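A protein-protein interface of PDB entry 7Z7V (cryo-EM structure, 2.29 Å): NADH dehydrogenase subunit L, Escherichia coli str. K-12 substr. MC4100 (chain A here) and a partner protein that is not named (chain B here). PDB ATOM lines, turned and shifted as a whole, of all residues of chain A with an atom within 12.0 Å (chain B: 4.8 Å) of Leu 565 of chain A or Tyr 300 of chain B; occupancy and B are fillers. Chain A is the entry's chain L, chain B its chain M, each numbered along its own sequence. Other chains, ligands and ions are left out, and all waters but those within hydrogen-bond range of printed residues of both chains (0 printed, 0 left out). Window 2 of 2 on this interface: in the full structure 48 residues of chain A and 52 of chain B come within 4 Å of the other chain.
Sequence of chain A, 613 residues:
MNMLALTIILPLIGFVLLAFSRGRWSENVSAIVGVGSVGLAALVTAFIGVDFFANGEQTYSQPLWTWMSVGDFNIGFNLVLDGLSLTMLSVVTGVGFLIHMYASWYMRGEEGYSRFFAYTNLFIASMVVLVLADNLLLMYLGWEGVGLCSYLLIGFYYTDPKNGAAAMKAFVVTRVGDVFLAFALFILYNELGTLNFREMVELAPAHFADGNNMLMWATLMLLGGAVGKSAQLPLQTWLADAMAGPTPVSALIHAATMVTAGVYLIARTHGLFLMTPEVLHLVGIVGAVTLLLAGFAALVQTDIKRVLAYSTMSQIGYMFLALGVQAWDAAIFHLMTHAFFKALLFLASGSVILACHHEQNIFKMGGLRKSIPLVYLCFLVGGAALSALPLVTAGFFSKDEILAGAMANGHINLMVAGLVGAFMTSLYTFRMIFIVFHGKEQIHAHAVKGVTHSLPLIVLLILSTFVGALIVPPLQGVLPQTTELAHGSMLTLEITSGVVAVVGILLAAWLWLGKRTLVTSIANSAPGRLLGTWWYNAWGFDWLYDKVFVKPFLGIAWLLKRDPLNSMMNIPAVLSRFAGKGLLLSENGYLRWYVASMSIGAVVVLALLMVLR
A ring nitrogen (NE2) of His 241 of chain B is in hydrogen-bond range of the side-chain carboxylate of Asp 563 of chain A, 3.1 Å away.
The side-chain hydroxyl of Tyr 300 of chain B lies within hydrogen-bond range of the backbone NH of Leu 565 of chain A, 3.2 Å away.
The backbone carbonyl oxygen (O) of Phe 553 of chain A lies within hydrogen-bond range of the indole nitrogen (NE1) of Trp 303 of chain B (3.1 Å).
The backbone carbonyl oxygen (O) of Leu 560 of chain A sits close to the side-chain sulfur (SD) of Met 304 of chain B (3.1 Å).
OD1 of Asp 563 of chain A sits close to OH of Tyr 300 of chain B (2.3 Å).
The backbone nitrogen (N) of Pro 564 of chain A sits close to the side-chain hydroxyl (OH) of Tyr 300 of chain B.
The backbone carbonyl oxygen of Asp 563 of chain A is in hydrogen-bond range of the side-chain hydroxyl of Ser 567 of chain A, at 3.5 Å.
Among the printed residues, pairs that only touch across the chains: Ile 556 of chain A with Trp 303 of chain B (3.5 Å), Ala 557 of chain A with Trp 303 of chain B (3.7 Å), Asp 563 of chain A with Met 304 of chain B (3.8 Å), Leu 565 of chain A with Pro 239 of chain B (3.9 Å), Met 568 of chain A with Pro 239 of chain B (3.7 Å) and Met 569 of chain A with Pro 239 of chain B (3.3 Å).
Printed residues of chain B within 4 Å of Asp 563 of chain A: His 241 (3.1 Å), Tyr 300 (2.3 Å) and Met 304 (3.8 Å).
Printed residues of chain B within 4 Å of Pro 564 of chain A: Tyr 300 (3.2 Å).
No residue of chain A comes within 4 Å of Val 238 of chain B.
Of chain A, only Leu 565 (3.9 Å), Met 568 (3.7 Å) and Met 569 (3.3 Å) come within 4 Å of Pro 239 of chain B.
Ile 296 of chain B touches none of the printed residues of chain A.
Gly 297 of chain B touches none of the printed residues of chain A.
Tyr 300 of chain B touches three residues of chain A.
No residue of chain A comes within 4 Å of Gly 301 of chain B.
No residue of chain A comes within 4 Å of Ala 302 of chain B.
Of the printed residues of chain A, Met 304 of chain B touches Leu 560 and Asp 563.
The nearest residue of chain B that does not touch Leu 565 of chain A is His 241 of chain B (4.1 Å).
The nearest printed residue of chain B that does not touch Phe 553 of chain A is Ala 302 of chain B (5.5 Å).
Hydrophobic or aromatic side chains of chain B within 4 Å of the printed part of chain A: Pro 239, His 241, Tyr 300, Trp 303 and Met 304.
Among the printed residues, no Asp or Glu carboxylate lies within 4 Å of a Lys or Arg side-chain nitrogen of the other chain.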
ATOM      1  N   PHE A 553     -33.108   6.851 -10.067  1.00  0.00           N
ATOM      2  CA  PHE A 553     -32.300   8.059  -9.914  1.00  0.00           C
ATOM      3  C   PHE A 553     -33.133   9.197  -9.341  1.00  0.00           C
ATOM      4  O   PHE A 553     -32.712   9.877  -8.396  1.00  0.00           O
ATOM      5  CB  PHE A 553     -31.688   8.469 -11.257  1.00  0.00           C
ATOM      6  CG  PHE A 553     -30.799   9.685 -11.178  1.00  0.00           C
ATOM      7  CD1 PHE A 553     -29.463   9.559 -10.849  1.00  0.00           C
ATOM      8  CD2 PHE A 553     -31.299  10.952 -11.438  1.00  0.00           C
ATOM      9  CE1 PHE A 553     -28.646  10.670 -10.775  1.00  0.00           C
ATOM     10  CE2 PHE A 553     -30.488  12.065 -11.359  1.00  0.00           C
ATOM     11  CZ  PHE A 553     -29.161  11.923 -11.030  1.00  0.00           C
ATOM     12  N   LEU A 554     -34.331   9.407  -9.892  1.00  0.00           N
ATOM     13  CA  LEU A 554     -35.209  10.455  -9.384  1.00  0.00           C
ATOM     14  C   LEU A 554     -35.695  10.138  -7.974  1.00  0.00           C
ATOM     15  O   LEU A 554     -35.836  11.043  -7.143  1.00  0.00           O
ATOM     16  CB  LEU A 554     -36.390  10.654 -10.332  1.00  0.00           C
ATOM     17  CG  LEU A 554     -36.039  11.177 -11.724  1.00  0.00           C
ATOM     18  CD1 LEU A 554     -37.281  11.276 -12.591  1.00  0.00           C
ATOM     19  CD2 LEU A 554     -35.342  12.517 -11.630  1.00  0.00           C
ATOM     20  N   GLY A 555     -35.936   8.858  -7.682  1.00  0.00           N
ATOM     21  CA  GLY A 555     -36.346   8.478  -6.343  1.00  0.00           C
ATOM     22  C   GLY A 555     -35.263   8.702  -5.306  1.00  0.00           C
ATOM     23  O   GLY A 555     -35.538   9.197  -4.212  1.00  0.00           O
ATOM     24  N   ILE A 556     -34.019   8.349  -5.637  1.00  0.00           N
ATOM     25  CA  ILE A 556     -32.908   8.570  -4.719  1.00  0.00           C
ATOM     26  C   ILE A 556     -32.638  10.061  -4.559  1.00  0.00           C
ATOM     27  O   ILE A 556     -32.308  10.526  -3.465  1.00  0.00           O
ATOM     28  CB  ILE A 556     -31.666   7.788  -5.191  1.00  0.00           C
ATOM     29  CG1 ILE A 556     -31.895   6.288  -5.013  1.00  0.00           C
ATOM     30  CG2 ILE A 556     -30.424   8.170  -4.407  1.00  0.00           C
ATOM     31  CD1 ILE A 556     -30.830   5.425  -5.641  1.00  0.00           C
ATOM     32  N   ALA A 557     -32.816  10.841  -5.631  1.00  0.00           N
ATOM     33  CA  ALA A 557     -32.683  12.291  -5.516  1.00  0.00           C
ATOM     34  C   ALA A 557     -33.735  12.878  -4.582  1.00  0.00           C
ATOM     35  O   ALA A 557     -33.421  13.721  -3.731  1.00  0.00           O
ATOM     36  CB  ALA A 557     -32.773  12.939  -6.896  1.00  0.00           C
ATOM     37  N   TRP A 558     -34.988  12.428  -4.714  1.00  0.00           N
ATOM     38  CA  TRP A 558     -36.052  12.898  -3.832  1.00  0.00           C
ATOM     39  C   TRP A 558     -35.812  12.461  -2.393  1.00  0.00           C
ATOM     40  O   TRP A 558     -36.100  13.210  -1.452  1.00  0.00           O
ATOM     41  CB  TRP A 558     -37.403  12.390  -4.328  1.00  0.00           C
ATOM     42  CG  TRP A 558     -38.547  12.729  -3.426  1.00  0.00           C
ATOM     43  CD1 TRP A 558     -39.299  13.866  -3.452  1.00  0.00           C
ATOM     44  CD2 TRP A 558     -39.070  11.927  -2.363  1.00  0.00           C
ATOM     45  NE1 TRP A 558     -40.257  13.821  -2.470  1.00  0.00           N
ATOM     46  CE2 TRP A 558     -40.137  12.641  -1.786  1.00  0.00           C
ATOM     47  CE3 TRP A 558     -38.737  10.674  -1.839  1.00  0.00           C
ATOM     48  CZ2 TRP A 558     -40.874  12.143  -0.717  1.00  0.00           C
ATOM     49  CZ3 TRP A 558     -39.468  10.182  -0.778  1.00  0.00           C
ATOM     50  CH2 TRP A 558     -40.525  10.915  -0.227  1.00  0.00           C
ATOM     51  N   LEU A 559     -35.295  11.249  -2.203  1.00  0.00           N
ATOM     52  CA  LEU A 559     -35.007  10.751  -0.865  1.00  0.00           C
ATOM     53  C   LEU A 559     -33.844  11.495  -0.221  1.00  0.00           C
ATOM     54  O   LEU A 559     -33.841  11.706   0.996  1.00  0.00           O
ATOM     55  CB  LEU A 559     -34.715   9.253  -0.934  1.00  0.00           C
ATOM     56  CG  LEU A 559     -34.393   8.500   0.353  1.00  0.00           C
ATOM     57  CD1 LEU A 559     -35.599   7.701   0.802  1.00  0.00           C
ATOM     58  CD2 LEU A 559     -33.197   7.595   0.141  1.00  0.00           C
ATOM     59  N   LEU A 560     -32.856  11.903  -1.014  1.00  0.00           N
ATOM     60  CA  LEU A 560     -31.653  12.527  -0.490  1.00  0.00           C
ATOM     61  C   LEU A 560     -31.731  14.043  -0.417  1.00  0.00           C
ATOM     62  O   LEU A 560     -30.865  14.644   0.222  1.00  0.00           O
ATOM     63  CB  LEU A 560     -30.443  12.138  -1.344  1.00  0.00           C
ATOM     64  CG  LEU A 560     -29.907  10.717  -1.188  1.00  0.00           C
ATOM     65  CD1 LEU A 560     -28.590  10.569  -1.923  1.00  0.00           C
ATOM     66  CD2 LEU A 560     -29.749  10.363   0.274  1.00  0.00           C
ATOM     67  N   LYS A 561     -32.751  14.669  -1.020  1.00  0.00           N
ATOM     68  CA  LYS A 561     -32.830  16.127  -1.130  1.00  0.00           C
ATOM     69  C   LYS A 561     -32.787  16.876   0.202  1.00  0.00           C
ATOM     70  O   LYS A 561     -32.586  18.095   0.191  1.00  0.00           O
ATOM     71  CB  LYS A 561     -34.104  16.519  -1.882  1.00  0.00           C
ATOM     72  CG  LYS A 561     -35.377  16.416  -1.067  1.00  0.00           C
ATOM     73  CD  LYS A 561     -36.518  17.153  -1.748  1.00  0.00           C
ATOM     74  CE  LYS A 561     -37.847  16.877  -1.063  1.00  0.00           C
ATOM     75  NZ  LYS A 561     -37.871  15.540  -0.400  1.00  0.00           N
ATOM     76  N   ARG A 562     -32.961  16.202   1.336  1.00  0.00           N
ATOM     77  CA  ARG A 562     -32.838  16.841   2.638  1.00  0.00           C
ATOM     78  C   ARG A 562     -31.444  16.718   3.243  1.00  0.00           C
ATOM     79  O   ARG A 562     -31.236  17.204   4.360  1.00  0.00           O
ATOM     80  CB  ARG A 562     -33.868  16.257   3.610  1.00  0.00           C
ATOM     81  CG  ARG A 562     -35.248  16.884   3.507  1.00  0.00           C
ATOM     82  CD  ARG A 562     -35.177  18.400   3.545  1.00  0.00           C
ATOM     83  NE  ARG A 562     -35.471  18.993   2.245  1.00  0.00           N
ATOM     84  CZ  ARG A 562     -36.692  19.210   1.777  1.00  0.00           C
ATOM     85  NH1 ARG A 562     -37.769  18.898   2.481  1.00  0.00           N
ATOM     86  NH2 ARG A 562     -36.839  19.755   0.573  1.00  0.00           N
ATOM     87  N   ASP A 563     -30.493  16.081   2.537  1.00  0.00           N
ATOM     88  CA  ASP A 563     -29.116  15.839   2.972  1.00  0.00           C
ATOM     89  C   ASP A 563     -29.070  15.066   4.287  1.00  0.00           C
ATOM     90  O   ASP A 563     -28.793  15.659   5.336  1.00  0.00           O
ATOM     91  CB  ASP A 563     -28.341  17.156   3.097  1.00  0.00           C
ATOM     92  CG  ASP A 563     -26.846  16.978   2.894  1.00  0.00           C
ATOM     93  OD1 ASP A 563     -26.347  15.851   3.063  1.00  0.00           O
ATOM     94  OD2 ASP A 563     -26.167  17.973   2.571  1.00  0.00           O
ATOM     95  N   PRO A 564     -29.370  13.761   4.276  1.00  0.00           N
ATOM     96  CA  PRO A 564     -29.399  12.992   5.536  1.00  0.00           C
ATOM     97  C   PRO A 564     -28.076  12.949   6.286  1.00  0.00           C
ATOM     98  O   PRO A 564     -28.086  12.896   7.523  1.00  0.00           O
ATOM     99  CB  PRO A 564     -29.819  11.589   5.078  1.00  0.00           C
ATOM    100  CG  PRO A 564     -30.413  11.773   3.733  1.00  0.00           C
ATOM    101  CD  PRO A 564     -29.697  12.918   3.116  1.00  0.00           C
ATOM    102  N   LEU A 565     -26.941  12.957   5.582  1.00  0.00           N
ATOM    103  CA  LEU A 565     -25.649  12.941   6.261  1.00  0.00           C
ATOM    104  C   LEU A 565     -25.405  14.231   7.033  1.00  0.00           C
ATOM    105  O   LEU A 565     -24.798  14.202   8.112  1.00  0.00           O
ATOM    106  CB  LEU A 565     -24.530  12.698   5.251  1.00  0.00           C
ATOM    107  CG  LEU A 565     -24.620  11.395   4.453  1.00  0.00           C
ATOM    108  CD1 LEU A 565     -23.435  11.256   3.520  1.00  0.00           C
ATOM    109  CD2 LEU A 565     -24.714  10.200   5.379  1.00  0.00           C
ATOM    110  N   ASN A 566     -25.886  15.359   6.507  1.00  0.00           N
ATOM    111  CA  ASN A 566     -25.797  16.625   7.225  1.00  0.00           C
ATOM    112  C   ASN A 566     -26.586  16.584   8.529  1.00  0.00           C
ATOM    113  O   ASN A 566     -26.118  17.076   9.559  1.00  0.00           O
ATOM    114  CB  ASN A 566     -26.292  17.762   6.331  1.00  0.00           C
ATOM    115  CG  ASN A 566     -26.152  19.120   6.982  1.00  0.00           C
ATOM    116  OD1 ASN A 566     -25.157  19.404   7.644  1.00  0.00           O
ATOM    117  ND2 ASN A 566     -27.156  19.966   6.802  1.00  0.00           N
ATOM    118  N   SER A 567     -27.780  15.985   8.512  1.00  0.00           N
ATOM    119  CA  SER A 567     -28.565  15.858   9.738  1.00  0.00           C
ATOM    120  C   SER A 567     -27.921  14.881  10.718  1.00  0.00           C
ATOM    121  O   SER A 567     -27.950  15.099  11.940  1.00  0.00           O
ATOM    122  CB  SER A 567     -29.989  15.420   9.402  1.00  0.00           C
ATOM    123  OG  SER A 567     -30.498  16.153   8.303  1.00  0.00           O
ATOM    124  N   MET A 568     -27.333  13.799  10.199  1.00  0.00           N
ATOM    125  CA  MET A 568     -26.648  12.841  11.060  1.00  0.00           C
ATOM    126  C   MET A 568     -25.451  13.485  11.750  1.00  0.00           C
ATOM    127  O   MET A 568     -25.163  13.190  12.915  1.00  0.00           O
ATOM    128  CB  MET A 568     -26.223  11.617  10.248  1.00  0.00           C
ATOM    129  CG  MET A 568     -25.486  10.555  11.047  1.00  0.00           C
ATOM    130  SD  MET A 568     -24.230   9.676  10.100  1.00  0.00           S
ATOM    131  CE  MET A 568     -23.318  11.042   9.400  1.00  0.00           C
ATOM    132  N   MET A 569     -24.755  14.383  11.056  1.00  0.00           N
ATOM    133  CA  MET A 569     -23.694  15.145  11.700  1.00  0.00           C
ATOM    134  C   MET A 569     -24.210  16.323  12.520  1.00  0.00           C
ATOM    135  O   MET A 569     -23.449  16.879  13.316  1.00  0.00           O
ATOM    136  CB  MET A 569     -22.696  15.644  10.656  1.00  0.00           C
ATOM    137  CG  MET A 569     -21.853  14.540  10.045  1.00  0.00           C
ATOM    138  SD  MET A 569     -20.945  13.578  11.268  1.00  0.00           S
ATOM    139  CE  MET A 569     -20.054  14.863  12.143  1.00  0.00           C
ATOM    140  N   ASN A 570     -25.466  16.730  12.332  1.00  0.00           N
ATOM    141  CA  ASN A 570     -26.077  17.740  13.188  1.00  0.00           C
ATOM    142  C   ASN A 570     -26.603  17.161  14.490  1.00  0.00           C
ATOM    143  O   ASN A 570     -26.973  17.928  15.385  1.00  0.00           O
ATOM    144  CB  ASN A 570     -27.223  18.434  12.451  1.00  0.00           C
ATOM    145  CG  ASN A 570     -26.819  19.767  11.872  1.00  0.00           C
ATOM    146  OD1 ASN A 570     -25.713  20.250  12.108  1.00  0.00           O
ATOM    147  ND2 ASN A 570     -27.716  20.375  11.105  1.00  0.00           N
ATOM    148  N   ILE A 571     -26.693  15.831  14.574  1.00  0.00           N
ATOM    149  CA  ILE A 571     -27.129  15.170  15.814  1.00  0.00           C
ATOM    150  C   ILE A 571     -26.346  15.601  17.066  1.00  0.00           C
ATOM    151  O   ILE A 571     -26.983  15.865  18.098  1.00  0.00           O
ATOM    152  CB  ILE A 571     -27.151  13.646  15.615  1.00  0.00           C
ATOM    153  CG1 ILE A 571     -28.416  13.223  14.870  1.00  0.00           C
ATOM    154  CG2 ILE A 571     -27.043  12.896  16.936  1.00  0.00           C
ATOM    155  CD1 ILE A 571     -28.366  11.808  14.354  1.00  0.00           C
ATOM    156  N   PRO A 572     -24.997  15.696  17.056  1.00  0.00           N
ATOM    157  CA  PRO A 572     -24.309  16.171  18.275  1.00  0.00           C
ATOM    158  C   PRO A 572     -24.681  17.581  18.711  1.00  0.00           C
ATOM    159  O   PRO A 572     -24.616  17.875  19.910  1.00  0.00           O
ATOM    160  CB  PRO A 572     -22.826  16.085  17.893  1.00  0.00           C
ATOM    161  CG  PRO A 572     -22.770  15.022  16.906  1.00  0.00           C
ATOM    162  CD  PRO A 572     -23.998  15.211  16.080  1.00  0.00           C
ATOM    163  N   ALA A 573     -25.080  18.456  17.787  1.00  0.00           N
ATOM    164  CA  ALA A 573     -25.537  19.785  18.181  1.00  0.00           C
ATOM    165  C   ALA A 573     -26.830  19.718  18.986  1.00  0.00           C
ATOM    166  O   ALA A 573     -26.971  20.410  20.002  1.00  0.00           O
ATOM    167  CB  ALA A 573     -25.725  20.668  16.949  1.00  0.00           C
ATOM    168  N   VAL A 574     -27.784  18.889  18.554  1.00  0.00           N
ATOM    169  CA  VAL A 574     -29.030  18.767  19.303  1.00  0.00           C
ATOM    170  C   VAL A 574     -28.788  18.031  20.617  1.00  0.00           C
ATOM    171  O   VAL A 574     -29.459  18.308  21.618  1.00  0.00           O
ATOM    172  CB  VAL A 574     -30.138  18.115  18.439  1.00  0.00           C
ATOM    173  CG1 VAL A 574     -29.875  18.350  16.959  1.00  0.00           C
ATOM    174  CG2 VAL A 574     -30.318  16.627  18.723  1.00  0.00           C
ATOM    175  N   VAL B 238     -17.448  13.602   2.630  1.00  0.00           N
ATOM    176  CA  VAL B 238     -18.688  13.204   3.307  1.00  0.00           C
ATOM    177  C   VAL B 238     -18.351  12.301   4.486  1.00  0.00           C
ATOM    178  O   VAL B 238     -17.396  11.503   4.401  1.00  0.00           O
ATOM    179  CB  VAL B 238     -19.645  12.504   2.325  1.00  0.00           C
ATOM    180  CG1 VAL B 238     -20.259  13.515   1.373  1.00  0.00           C
ATOM    181  CG2 VAL B 238     -18.927  11.417   1.553  1.00  0.00           C
ATOM    182  N   PRO B 239     -19.061  12.391   5.620  1.00  0.00           N
ATOM    183  CA  PRO B 239     -20.204  13.270   5.880  1.00  0.00           C
ATOM    184  C   PRO B 239     -19.850  14.630   6.481  1.00  0.00           C
ATOM    185  O   PRO B 239     -20.740  15.305   6.989  1.00  0.00           O
ATOM    186  CB  PRO B 239     -21.028  12.453   6.869  1.00  0.00           C
ATOM    187  CG  PRO B 239     -20.010  11.698   7.646  1.00  0.00           C
ATOM    188  CD  PRO B 239     -18.809  11.489   6.756  1.00  0.00           C
ATOM    189  N   HIS B 241     -19.372  17.548   5.287  1.00  0.00           N
ATOM    190  CA  HIS B 241     -19.540  18.465   4.172  1.00  0.00           C
ATOM    191  C   HIS B 241     -20.670  19.459   4.359  1.00  0.00           C
ATOM    192  O   HIS B 241     -20.744  20.423   3.589  1.00  0.00           O
ATOM    193  CB  HIS B 241     -19.816  17.682   2.882  1.00  0.00           C
ATOM    194  CG  HIS B 241     -21.217  17.169   2.799  1.00  0.00           C
ATOM    195  ND1 HIS B 241     -21.654  16.087   3.534  1.00  0.00           N
ATOM    196  CD2 HIS B 241     -22.291  17.609   2.105  1.00  0.00           C
ATOM    197  CE1 HIS B 241     -22.931  15.875   3.280  1.00  0.00           C
ATOM    198  NE2 HIS B 241     -23.341  16.784   2.417  1.00  0.00           N
ATOM    199  N   ILE B 296     -18.282   7.725  -2.494  1.00  0.00           N
ATOM    200  CA  ILE B 296     -19.525   8.175  -1.879  1.00  0.00           C
ATOM    201  C   ILE B 296     -19.672   9.682  -2.031  1.00  0.00           C
ATOM    202  O   ILE B 296     -20.766  10.183  -2.292  1.00  0.00           O
ATOM    203  CB  ILE B 296     -19.578   7.733  -0.403  1.00  0.00           C
ATOM    204  CG1 ILE B 296     -19.710   6.214  -0.310  1.00  0.00           C
ATOM    205  CG2 ILE B 296     -20.741   8.374   0.331  1.00  0.00           C
ATOM    206  CD1 ILE B 296     -19.378   5.666   1.051  1.00  0.00           C
ATOM    207  N   GLY B 297     -18.567  10.421  -1.921  1.00  0.00           N
ATOM    208  CA  GLY B 297     -18.624  11.858  -2.115  1.00  0.00           C
ATOM    209  C   GLY B 297     -19.010  12.249  -3.525  1.00  0.00           C
ATOM    210  O   GLY B 297     -19.828  13.148  -3.718  1.00  0.00           O
ATOM    211  N   ILE B 298     -18.462  11.546  -4.523  1.00  0.00           N
ATOM    212  CA  ILE B 298     -18.794  11.816  -5.921  1.00  0.00           C
ATOM    213  C   ILE B 298     -20.285  11.628  -6.160  1.00  0.00           C
ATOM    214  O   ILE B 298     -20.982  12.543  -6.622  1.00  0.00           O
ATOM    215  CB  ILE B 298     -17.970  10.904  -6.851  1.00  0.00           C
ATOM    216  CG1 ILE B 298     -16.502  11.317  -6.868  1.00  0.00           C
ATOM    217  CG2 ILE B 298     -18.534  10.921  -8.261  1.00  0.00           C
ATOM    218  CD1 ILE B 298     -15.609  10.292  -7.498  1.00  0.00           C
ATOM    219  N   PHE B 299     -20.812  10.465  -5.776  1.00  0.00           N
ATOM    220  CA  PHE B 299     -22.212  10.191  -6.088  1.00  0.00           C
ATOM    221  C   PHE B 299     -23.181  10.957  -5.200  1.00  0.00           C
ATOM    222  O   PHE B 299     -24.213  11.439  -5.683  1.00  0.00           O
ATOM    223  CB  PHE B 299     -22.468   8.695  -6.032  1.00  0.00           C
ATOM    224  CG  PHE B 299     -21.945   7.990  -7.220  1.00  0.00           C
ATOM    225  CD1 PHE B 299     -20.682   7.446  -7.223  1.00  0.00           C
ATOM    226  CD2 PHE B 299     -22.710   7.919  -8.366  1.00  0.00           C
ATOM    227  CE1 PHE B 299     -20.205   6.830  -8.342  1.00  0.00           C
ATOM    228  CE2 PHE B 299     -22.241   7.297  -9.483  1.00  0.00           C
ATOM    229  CZ  PHE B 299     -20.995   6.749  -9.472  1.00  0.00           C
ATOM    230  N   TYR B 300     -22.864  11.089  -3.913  1.00  0.00           N
ATOM    231  CA  TYR B 300     -23.693  11.863  -3.004  1.00  0.00           C
ATOM    232  C   TYR B 300     -23.741  13.326  -3.410  1.00  0.00           C
ATOM    233  O   TYR B 300     -24.819  13.923  -3.441  1.00  0.00           O
ATOM    234  CB  TYR B 300     -23.162  11.710  -1.581  1.00  0.00           C
ATOM    235  CG  TYR B 300     -24.086  12.227  -0.514  1.00  0.00           C
ATOM    236  CD1 TYR B 300     -25.118  11.441  -0.024  1.00  0.00           C
ATOM    237  CD2 TYR B 300     -23.921  13.499   0.011  1.00  0.00           C
ATOM    238  CE1 TYR B 300     -25.962  11.911   0.953  1.00  0.00           C
ATOM    239  CE2 TYR B 300     -24.758  13.978   0.987  1.00  0.00           C
ATOM    240  CZ  TYR B 300     -25.777  13.181   1.454  1.00  0.00           C
ATOM    241  OH  TYR B 300     -26.611  13.659   2.429  1.00  0.00           O
ATOM    242  N   GLY B 301     -22.591  13.916  -3.747  1.00  0.00           N
ATOM    243  CA  GLY B 301     -22.578  15.297  -4.185  1.00  0.00           C
ATOM    244  C   GLY B 301     -23.307  15.503  -5.496  1.00  0.00           C
ATOM    245  O   GLY B 301     -23.976  16.519  -5.680  1.00  0.00           O
ATOM    246  N   ALA B 302     -23.203  14.538  -6.418  1.00  0.00           N
ATOM    247  CA  ALA B 302     -23.949  14.647  -7.668  1.00  0.00           C
ATOM    248  C   ALA B 302     -25.456  14.589  -7.433  1.00  0.00           C
ATOM    249  O   ALA B 302     -26.209  15.396  -7.999  1.00  0.00           O
ATOM    250  CB  ALA B 302     -23.512  13.549  -8.632  1.00  0.00           C
ATOM    251  N   TRP B 303     -25.909  13.656  -6.591  1.00  0.00           N
ATOM    252  CA  TRP B 303     -27.334  13.549  -6.295  1.00  0.00           C
ATOM    253  C   TRP B 303     -27.844  14.775  -5.547  1.00  0.00           C
ATOM    254  O   TRP B 303     -28.958  15.245  -5.805  1.00  0.00           O
ATOM    255  CB  TRP B 303     -27.609  12.282  -5.491  1.00  0.00           C
ATOM    256  CG  TRP B 303     -28.265  11.216  -6.294  1.00  0.00           C
ATOM    257  CD1 TRP B 303     -29.384  11.342  -7.059  1.00  0.00           C
ATOM    258  CD2 TRP B 303     -27.844   9.856  -6.417  1.00  0.00           C
ATOM    259  NE1 TRP B 303     -29.690  10.144  -7.650  1.00  0.00           N
ATOM    260  CE2 TRP B 303     -28.756   9.215  -7.275  1.00  0.00           C
ATOM    261  CE3 TRP B 303     -26.784   9.117  -5.885  1.00  0.00           C
ATOM    262  CZ2 TRP B 303     -28.644   7.870  -7.610  1.00  0.00           C
ATOM    263  CZ3 TRP B 303     -26.673   7.787  -6.221  1.00  0.00           C
ATOM    264  CH2 TRP B 303     -27.597   7.175  -7.074  1.00  0.00           C
ATOM    265  N   MET B 304     -27.047  15.301  -4.616  1.00  0.00           N
ATOM    266  CA  MET B 304     -27.423  16.519  -3.908  1.00  0.00           C
ATOM    267  C   MET B 304     -27.483  17.714  -4.848  1.00  0.00           C
ATOM    268  O   MET B 304     -28.364  18.567  -4.709  1.00  0.00           O
ATOM    269  CB  MET B 304     -26.440  16.800  -2.769  1.00  0.00           C
ATOM    270  CG  MET B 304     -26.478  15.866  -1.573  1.00  0.00           C
ATOM    271  SD  MET B 304     -28.062  15.552  -0.791  1.00  0.00           S
ATOM    272  CE  MET B 304     -28.782  17.190  -0.653  1.00  0.00           C
